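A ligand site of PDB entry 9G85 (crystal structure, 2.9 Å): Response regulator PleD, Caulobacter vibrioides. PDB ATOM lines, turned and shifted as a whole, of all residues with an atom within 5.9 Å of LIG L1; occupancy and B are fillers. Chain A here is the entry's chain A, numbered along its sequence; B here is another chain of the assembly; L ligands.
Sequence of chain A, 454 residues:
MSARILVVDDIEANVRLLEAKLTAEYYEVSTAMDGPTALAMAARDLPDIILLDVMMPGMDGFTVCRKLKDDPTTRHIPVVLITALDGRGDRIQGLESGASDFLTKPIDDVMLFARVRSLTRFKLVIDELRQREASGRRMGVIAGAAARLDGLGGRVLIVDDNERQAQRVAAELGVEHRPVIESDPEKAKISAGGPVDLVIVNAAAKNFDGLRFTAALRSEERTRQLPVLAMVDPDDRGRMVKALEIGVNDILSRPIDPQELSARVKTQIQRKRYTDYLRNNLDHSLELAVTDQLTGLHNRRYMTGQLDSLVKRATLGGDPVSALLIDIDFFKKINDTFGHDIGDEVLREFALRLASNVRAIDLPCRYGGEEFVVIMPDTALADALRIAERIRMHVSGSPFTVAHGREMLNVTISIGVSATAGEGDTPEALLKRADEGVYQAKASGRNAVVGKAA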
ATOM      1  N   ASN A 357       8.923   6.967 -27.366  1.00  0.00           N
ATOM      2  CA  ASN A 357       7.840   7.613 -26.640  1.00  0.00           C
ATOM      3  C   ASN A 357       7.962   9.132 -26.597  1.00  0.00           C
ATOM      4  O   ASN A 357       7.317   9.781 -25.769  1.00  0.00           O
ATOM      5  CB  ASN A 357       7.741   7.029 -25.227  1.00  0.00           C
ATOM      6  CG  ASN A 357       7.177   5.632 -25.228  1.00  0.00           C
ATOM      7  OD1 ASN A 357       5.962   5.443 -25.250  1.00  0.00           O
ATOM      8  ND2 ASN A 357       8.062   4.645 -25.220  1.00  0.00           N
ATOM      9  N   VAL A 358       8.780   9.710 -27.470  1.00  0.00           N
ATOM     10  CA  VAL A 358       8.809  11.150 -27.677  1.00  0.00           C
ATOM     11  C   VAL A 358       8.805  11.395 -29.188  1.00  0.00           C
ATOM     12  O   VAL A 358       9.094  10.500 -29.986  1.00  0.00           O
ATOM     13  CB  VAL A 358      10.019  11.844 -27.025  1.00  0.00           C
ATOM     14  CG1 VAL A 358       9.884  11.818 -25.502  1.00  0.00           C
ATOM     15  CG2 VAL A 358      11.326  11.208 -27.470  1.00  0.00           C
ATOM     16  N   ARG A 359       8.447  12.622 -29.570  1.00  0.00           N
ATOM     17  CA  ARG A 359       8.337  12.945 -30.981  1.00  0.00           C
ATOM     18  C   ARG A 359       9.703  12.925 -31.658  1.00  0.00           C
ATOM     19  O   ARG A 359      10.732  13.230 -31.040  1.00  0.00           O
ATOM     20  CB  ARG A 359       7.702  14.326 -31.164  1.00  0.00           C
ATOM     21  CG  ARG A 359       6.265  14.403 -30.714  1.00  0.00           C
ATOM     22  CD  ARG A 359       5.684  15.773 -30.956  1.00  0.00           C
ATOM     23  NE  ARG A 359       4.291  15.839 -30.524  1.00  0.00           N
ATOM     24  CZ  ARG A 359       3.528  16.911 -30.676  1.00  0.00           C
ATOM     25  NH1 ARG A 359       3.980  18.017 -31.243  1.00  0.00           N
ATOM     26  NH2 ARG A 359       2.261  16.858 -30.250  1.00  0.00           N
ATOM     27  N   ILE A 361      10.607  15.053 -33.682  1.00  0.00           N
ATOM     28  CA  ILE A 361      11.083  16.437 -33.664  1.00  0.00           C
ATOM     29  C   ILE A 361      11.760  16.784 -32.347  1.00  0.00           C
ATOM     30  O   ILE A 361      12.481  17.790 -32.276  1.00  0.00           O
ATOM     31  CB  ILE A 361       9.923  17.413 -33.934  1.00  0.00           C
ATOM     32  CG1 ILE A 361       9.015  17.529 -32.708  1.00  0.00           C
ATOM     33  CG2 ILE A 361       9.144  16.976 -35.157  1.00  0.00           C
ATOM     34  CD1 ILE A 361       7.938  18.585 -32.850  1.00  0.00           C
ATOM     35  N   ASP A 362      11.541  15.990 -31.302  1.00  0.00           N
ATOM     36  CA  ASP A 362      12.243  16.194 -30.056  1.00  0.00           C
ATOM     37  C   ASP A 362      13.688  15.696 -30.189  1.00  0.00           C
ATOM     38  O   ASP A 362      14.046  15.025 -31.156  1.00  0.00           O
ATOM     39  CB  ASP A 362      11.526  15.485 -28.905  1.00  0.00           C
ATOM     40  CG  ASP A 362      10.105  15.987 -28.718  1.00  0.00           C
ATOM     41  OD1 ASP A 362       9.873  17.209 -28.838  1.00  0.00           O
ATOM     42  OD2 ASP A 362       9.213  15.152 -28.431  1.00  0.00           O
ATOM     43  N   MET A 376      12.518  19.515 -25.953  1.00  0.00           N
ATOM     44  CA  MET A 376      11.196  19.512 -26.574  1.00  0.00           C
ATOM     45  C   MET A 376      10.861  20.922 -27.014  1.00  0.00           C
ATOM     46  O   MET A 376      10.427  21.747 -26.203  1.00  0.00           O
ATOM     47  CB  MET A 376      10.155  18.967 -25.590  1.00  0.00           C
ATOM     48  CG  MET A 376      10.354  17.475 -25.317  1.00  0.00           C
ATOM     49  SD  MET A 376       9.258  16.786 -24.061  1.00  0.00           S
ATOM     50  CE  MET A 376       9.408  18.033 -22.782  1.00  0.00           C
ATOM     51  N   PRO A 377      11.043  21.246 -28.289  1.00  0.00           N
ATOM     52  CA  PRO A 377      10.767  22.603 -28.753  1.00  0.00           C
ATOM     53  C   PRO A 377       9.272  22.880 -28.823  1.00  0.00           C
ATOM     54  O   PRO A 377       8.455  21.961 -28.994  1.00  0.00           O
ATOM     55  CB  PRO A 377      11.395  22.642 -30.147  1.00  0.00           C
ATOM     56  CG  PRO A 377      11.320  21.214 -30.615  1.00  0.00           C
ATOM     57  CD  PRO A 377      11.509  20.363 -29.382  1.00  0.00           C
ATOM     58  N   ASP A 378       8.918  24.157 -28.663  1.00  0.00           N
ATOM     59  CA  ASP A 378       7.531  24.610 -28.713  1.00  0.00           C
ATOM     60  C   ASP A 378       6.665  23.843 -27.732  1.00  0.00           C
ATOM     61  O   ASP A 378       5.614  23.291 -28.076  1.00  0.00           O
ATOM     62  CB  ASP A 378       6.981  24.512 -30.137  1.00  0.00           C
ATOM     63  CG  ASP A 378       7.815  25.273 -31.149  1.00  0.00           C
ATOM     64  OD1 ASP A 378       8.105  26.467 -30.907  1.00  0.00           O
ATOM     65  OD2 ASP A 378       8.160  24.681 -32.195  1.00  0.00           O
ATOM     66  N   THR A 379       7.114  23.795 -26.482  1.00  0.00           N
ATOM     67  CA  THR A 379       6.455  23.004 -25.446  1.00  0.00           C
ATOM     68  C   THR A 379       6.527  23.737 -24.116  1.00  0.00           C
ATOM     69  O   THR A 379       7.570  24.295 -23.762  1.00  0.00           O
ATOM     70  CB  THR A 379       7.116  21.621 -25.319  1.00  0.00           C
ATOM     71  OG1 THR A 379       7.191  21.007 -26.607  1.00  0.00           O
ATOM     72  CG2 THR A 379       6.308  20.732 -24.385  1.00  0.00           C
ATOM     73  N   ASP A 383       2.903  20.732 -20.009  1.00  0.00           N
ATOM     74  CA  ASP A 383       2.916  19.547 -20.861  1.00  0.00           C
ATOM     75  C   ASP A 383       4.173  18.718 -20.621  1.00  0.00           C
ATOM     76  O   ASP A 383       4.103  17.479 -20.548  1.00  0.00           O
ATOM     77  CB  ASP A 383       2.818  19.959 -22.326  1.00  0.00           C
ATOM     78  CG  ASP A 383       1.447  20.487 -22.691  1.00  0.00           C
ATOM     79  OD1 ASP A 383       0.500  20.283 -21.896  1.00  0.00           O
ATOM     80  OD2 ASP A 383       1.311  21.124 -23.763  1.00  0.00           O
ATOM     81  N   ARG A 386       3.755  16.328 -17.882  1.00  0.00           N
ATOM     82  CA  ARG A 386       2.942  15.165 -18.231  1.00  0.00           C
ATOM     83  C   ARG A 386       3.671  14.236 -19.186  1.00  0.00           C
ATOM     84  O   ARG A 386       3.430  13.024 -19.172  1.00  0.00           O
ATOM     85  CB  ARG A 386       1.612  15.624 -18.836  1.00  0.00           C
ATOM     86  CG  ARG A 386       0.833  16.590 -17.947  1.00  0.00           C
ATOM     87  CD  ARG A 386      -0.565  16.853 -18.473  1.00  0.00           C
ATOM     88  NE  ARG A 386      -0.557  17.396 -19.821  1.00  0.00           N
ATOM     89  CZ  ARG A 386      -0.955  16.742 -20.901  1.00  0.00           C
ATOM     90  NH1 ARG A 386      -1.409  15.497 -20.821  1.00  0.00           N
ATOM     91  NH2 ARG A 386      -0.896  17.345 -22.087  1.00  0.00           N
ATOM     92  N   ILE A 387       4.571  14.774 -20.024  1.00  0.00           N
ATOM     93  CA  ILE A 387       5.353  13.923 -20.913  1.00  0.00           C
ATOM     94  C   ILE A 387       6.361  13.099 -20.107  1.00  0.00           C
ATOM     95  O   ILE A 387       6.541  11.907 -20.367  1.00  0.00           O
ATOM     96  CB  ILE A 387       6.051  14.771 -21.987  1.00  0.00           C
ATOM     97  CG1 ILE A 387       5.032  15.509 -22.843  1.00  0.00           C
ATOM     98  CG2 ILE A 387       6.904  13.885 -22.889  1.00  0.00           C
ATOM     99  CD1 ILE A 387       5.623  16.679 -23.597  1.00  0.00           C
ATOM    100  N   ARG A 390       4.677  10.235 -18.799  1.00  0.00           N
ATOM    101  CA  ARG A 390       4.522   9.194 -19.814  1.00  0.00           C
ATOM    102  C   ARG A 390       5.796   8.370 -19.928  1.00  0.00           C
ATOM    103  O   ARG A 390       5.740   7.141 -20.013  1.00  0.00           O
ATOM    104  CB  ARG A 390       4.220   9.794 -21.176  1.00  0.00           C
ATOM    105  CG  ARG A 390       4.032   8.705 -22.230  1.00  0.00           C
ATOM    106  CD  ARG A 390       3.981   9.257 -23.636  1.00  0.00           C
ATOM    107  NE  ARG A 390       3.392  10.583 -23.699  1.00  0.00           N
ATOM    108  CZ  ARG A 390       3.801  11.537 -24.528  1.00  0.00           C
ATOM    109  NH1 ARG A 390       4.816  11.342 -25.364  1.00  0.00           N
ATOM    110  NH2 ARG A 390       3.174  12.707 -24.521  1.00  0.00           N
ATOM    111  N   ARG B 178       4.931  18.030 -38.367  1.00  0.00           N
ATOM    112  CA  ARG B 178       4.791  18.957 -37.250  1.00  0.00           C
ATOM    113  C   ARG B 178       5.090  20.356 -37.796  1.00  0.00           C
ATOM    114  O   ARG B 178       6.238  20.811 -37.760  1.00  0.00           O
ATOM    115  CB  ARG B 178       5.758  18.587 -36.133  1.00  0.00           C
ATOM    116  CG  ARG B 178       5.594  17.163 -35.595  1.00  0.00           C
ATOM    117  CD  ARG B 178       4.315  16.877 -34.838  1.00  0.00           C
ATOM    118  NE  ARG B 178       4.341  15.500 -34.353  1.00  0.00           N
ATOM    119  CZ  ARG B 178       3.362  14.903 -33.679  1.00  0.00           C
ATOM    120  NH1 ARG B 178       2.233  15.531 -33.392  1.00  0.00           N
ATOM    121  NH2 ARG B 178       3.527  13.644 -33.293  1.00  0.00           N
HETATM  122  P1  LIG L   1      -0.793  18.918 -29.763  1.00  0.00           P
HETATM  123  O1  LIG L   1      -1.859  19.707 -30.489  1.00  0.00           O
HETATM  124  O2  LIG L   1       0.330  18.831 -30.763  1.00  0.00           O
HETATM  125  O3  LIG L   1      -1.542  17.462 -29.366  1.00  0.00           O
HETATM  126  C1  LIG L   1      -2.974  17.455 -29.070  1.00  0.00           C
HETATM  127  C2  LIG L   1      -3.442  15.996 -28.795  1.00  0.00           C
HETATM  128  O4  LIG L   1      -3.296  15.104 -30.136  1.00  0.00           O
HETATM  129  C3  LIG L   1      -2.678  15.479 -27.977  1.00  0.00           C
HETATM  130  O5  LIG L   1      -3.208  15.697 -26.525  1.00  0.00           O
HETATM  131  C4  LIG L   1      -2.629  13.955 -28.349  1.00  0.00           C
HETATM  132  O6  LIG L   1      -3.719  13.413 -27.760  1.00  0.00           O
HETATM  133  C5  LIG L   1      -2.810  13.928 -29.835  1.00  0.00           C
HETATM  134  N1  LIG L   1      -1.500  13.766 -30.550  1.00  0.00           N
HETATM  135  C6  LIG L   1      -0.736  14.635 -31.229  1.00  0.00           C
HETATM  136  N2  LIG L   1       0.344  13.954 -31.690  1.00  0.00           N
HETATM  137  C7  LIG L   1       0.186  12.678 -31.272  1.00  0.00           C
HETATM  138  C8  LIG L   1       1.040  11.428 -31.450  1.00  0.00           C
HETATM  139  O7  LIG L   1       2.046  11.498 -32.062  1.00  0.00           O
HETATM  140  N3  LIG L   1       0.664  10.150 -30.899  1.00  0.00           N
HETATM  141  C9  LIG L   1      -0.548  10.039 -30.142  1.00  0.00           C
HETATM  142  N4  LIG L   1      -0.954   8.763 -29.577  1.00  0.00           N
HETATM  143  N5  LIG L   1      -1.367  11.235 -29.967  1.00  0.00           N
HETATM  144  C10 LIG L   1      -0.966  12.554 -30.550  1.00  0.00           C
HETATM  145  P2  LIG L   1      -1.930  15.496 -25.363  1.00  0.00           P
HETATM  146  O8  LIG L   1      -2.401  16.038 -24.031  1.00  0.00           O
HETATM  147  O9  LIG L   1      -1.474  14.088 -25.082  1.00  0.00           O
HETATM  148  O10 LIG L   1      -0.802  16.575 -26.026  1.00  0.00           O
HETATM  149  C11 LIG L   1      -1.126  17.982 -25.707  1.00  0.00           C
HETATM  150  C12 LIG L   1      -0.050  18.985 -26.199  1.00  0.00           C
HETATM  151  O11 LIG L   1       1.295  18.654 -25.332  1.00  0.00           O
HETATM  152  C13 LIG L   1       0.256  18.741 -27.377  1.00  0.00           C
HETATM  153  O12 LIG L   1      -0.379  19.795 -28.342  1.00  0.00           O
HETATM  154  C14 LIG L   1       1.803  18.945 -27.484  1.00  0.00           C
HETATM  155  O13 LIG L   1       2.011  20.257 -27.739  1.00  0.00           O
HETATM  156  C15 LIG L   1       2.329  18.574 -26.125  1.00  0.00           C
HETATM  157  N6  LIG L   1       2.886  17.179 -26.186  1.00  0.00           N
HETATM  158  C16 LIG L   1       2.326  16.031 -25.775  1.00  0.00           C
HETATM  159  N7  LIG L   1       3.189  15.030 -26.007  1.00  0.00           N
HETATM  160  C17 LIG L   1       4.276  15.575 -26.561  1.00  0.00           C
HETATM  161  C18 LIG L   1       5.603  14.991 -27.057  1.00  0.00           C
HETATM  162  O14 LIG L   1       5.780  13.827 -26.959  1.00  0.00           O
HETATM  163  N8  LIG L   1       6.647  15.802 -27.636  1.00  0.00           N
HETATM  164  C19 LIG L   1       6.455  17.207 -27.755  1.00  0.00           C
HETATM  165  N9  LIG L   1       7.479  18.071 -28.330  1.00  0.00           N
HETATM  166  N10 LIG L   1       5.179  17.776 -27.271  1.00  0.00           N
HETATM  167  C20 LIG L   1       4.104  16.934 -26.679  1.00  0.00           C
HETATM  168  P1  LG2 L   2       2.422   7.022 -31.950  1.00  0.00           P
HETATM  169  O1  LG2 L   2       2.249   5.671 -32.580  1.00  0.00           O
HETATM  170  O2  LG2 L   2       1.065   7.354 -31.396  1.00  0.00           O
HETATM  171  O3  LG2 L   2       2.932   8.027 -33.190  1.00  0.00           O
HETATM  172  C1  LG2 L   2       3.694   7.434 -34.292  1.00  0.00           C
HETATM  173  C2  LG2 L   2       3.937   8.510 -35.388  1.00  0.00           C
HETATM  174  O4  LG2 L   2       2.532   8.876 -36.118  1.00  0.00           O
HETATM  175  C3  LG2 L   2       4.303   9.549 -34.826  1.00  0.00           C
HETATM  176  O5  LG2 L   2       5.861   9.617 -34.692  1.00  0.00           O
HETATM  177  C4  LG2 L   2       3.733  10.716 -35.704  1.00  0.00           C
HETATM  178  O6  LG2 L   2       4.580  10.871 -36.741  1.00  0.00           O
HETATM  179  C5  LG2 L   2       2.437  10.187 -36.247  1.00  0.00           C
HETATM  180  N1  LG2 L   2       1.254  10.657 -35.459  1.00  0.00           N
HETATM  181  C6  LG2 L   2       0.418  10.004 -34.639  1.00  0.00           C
HETATM  182  N2  LG2 L   2      -0.506  10.886 -34.220  1.00  0.00           N
HETATM  183  C7  LG2 L   2      -0.213  12.063 -34.820  1.00  0.00           C
HETATM  184  C8  LG2 L   2      -0.869  13.444 -34.761  1.00  0.00           C
HETATM  185  O7  LG2 L   2      -1.829  13.581 -34.083  1.00  0.00           O
HETATM  186  N3  LG2 L   2      -0.374  14.574 -35.490  1.00  0.00           N
HETATM  187  C9  LG2 L   2       0.790  14.421 -36.312  1.00  0.00           C
HETATM  188  N4  LG2 L   2       1.323  15.552 -37.061  1.00  0.00           N
HETATM  189  N5  LG2 L   2       1.425  13.094 -36.367  1.00  0.00           N
HETATM  190  C10 LG2 L   2       0.898  11.936 -35.608  1.00  0.00           C
HETATM  191  P2  LG2 L   2       6.314  10.728 -33.419  1.00  0.00           P
HETATM  192  O8  LG2 L   2       7.780  10.538 -33.098  1.00  0.00           O
HETATM  193  O9  LG2 L   2       6.174  12.192 -33.720  1.00  0.00           O
HETATM  194  O10 LG2 L   2       5.380  10.099 -32.138  1.00  0.00           O
HETATM  195  C11 LG2 L   2       6.044   8.929 -31.514  1.00  0.00           C
HETATM  196  C12 LG2 L   2       5.292   8.395 -30.267  1.00  0.00           C
HETATM  197  O11 LG2 L   2       5.468   9.497 -29.076  1.00  0.00           O
HETATM  198  C13 LG2 L   2       4.066   8.329 -30.466  1.00  0.00           C
HETATM  199  O12 LG2 L   2       3.641   6.867 -30.751  1.00  0.00           O
HETATM  200  C14 LG2 L   2       3.391   8.689 -29.110  1.00  0.00           C
HETATM  201  O13 LG2 L   2       3.393   7.555 -28.384  1.00  0.00           O
HETATM  202  C15 LG2 L   2       4.313   9.698 -28.503  1.00  0.00           C
HETATM  203  N6  LG2 L   2       3.781  11.069 -28.805  1.00  0.00           N
HETATM  204  C16 LG2 L   2       4.276  11.987 -29.647  1.00  0.00           C
HETATM  205  N7  LG2 L   2       3.509  13.095 -29.598  1.00  0.00           N
HETATM  206  C17 LG2 L   2       2.545  12.831 -28.700  1.00  0.00           C
HETATM  207  C18 LG2 L   2       1.362  13.644 -28.174  1.00  0.00           C
HETATM  208  O14 LG2 L   2       1.199  14.742 -28.603  1.00  0.00           O
HETATM  209  N8  LG2 L   2       0.443  13.149 -27.191  1.00  0.00           N
HETATM  210  C19 LG2 L   2       0.637  11.829 -26.673  1.00  0.00           C
HETATM  211  N9  LG2 L   2      -0.270  11.278 -25.671  1.00  0.00           N
HETATM  212  N10 LG2 L   2       1.762  11.036 -27.177  1.00  0.00           N
HETATM  213  C20 LG2 L   2       2.712  11.569 -28.185  1.00  0.00           C
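OD2 of Asp 362 is in hydrogen-bond range of N of Arg 359. O of Asn 357 sits at hydrogen-bond distance from NH1 of Arg 390, 3.0 Å away. NH2 of Arg 386 lies within salt-bridge range of OD1 of Asp 383. O of Met 376 sits at hydrogen-bond distance from OG1 of Thr 379. OG1 of Thr 379 sits at hydrogen-bond distance from O of Pro 377 (2.9 Å).
A nitrogen (N9) of LIG L1 sits at hydrogen-bond distance from the side-chain carboxylate (OD1) of Asp 362, at 2.6 Å. The guanidinium group (NH2) of Arg 390 is in hydrogen-bond range of a nitrogen (N7) of LIG L1 (2.8 Å). The guanidinium group of Arg 386 lies within salt-bridge range of an oxygen (O8) of LIG L1, at 2.8 Å. An oxygen (O2) of LIG L1 is in salt-bridge range of the guanidinium group (NH2) of Arg 359, at 2.8 Å. NH2 of Arg 178 of chain B sits at hydrogen-bond distance from O7 of LIG L1, 2.9 Å away. N9 of LIG L1 sits at hydrogen-bond distance from OG1 of Thr 379 (3.4 Å). The guanidinium group (NH2) of Arg 390 lies close to a nitrogen (N10) of LG2 L2, 3.4 Å away. NH2 of Arg 359 is in hydrogen-bond range of O14 of LG2 L2, at 2.9 Å. NH2 of Arg 178 of chain B lies within salt-bridge range of O9 of LG2 L2 (3.0 Å).
An oxygen (O2) of LG2 L2 lies within hydrogen-bond range of a nitrogen (N3) of LIG L1 (2.9 Å).
An oxygen (O11) of LIG L1 lies close to the side-chain carboxylate of Asp 383, 2.9 Å away. Residues that only touch LIG L1: Ile 387 (3.4 Å) and Met 376 (3.9 Å). Hydrophobic or aromatic side chains within 4 Å of LIG L1: Met 376 and Ile 387. Within 4 Å of LIG L1: Arg 359, Asp 362, Met 376, Thr 379, Asp 383, Arg 386, Ile 387, Arg 390 and Arg 178 of chain B. The nearest printed residue that does not touch LIG L1 is Pro 377 (4.1 Å).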
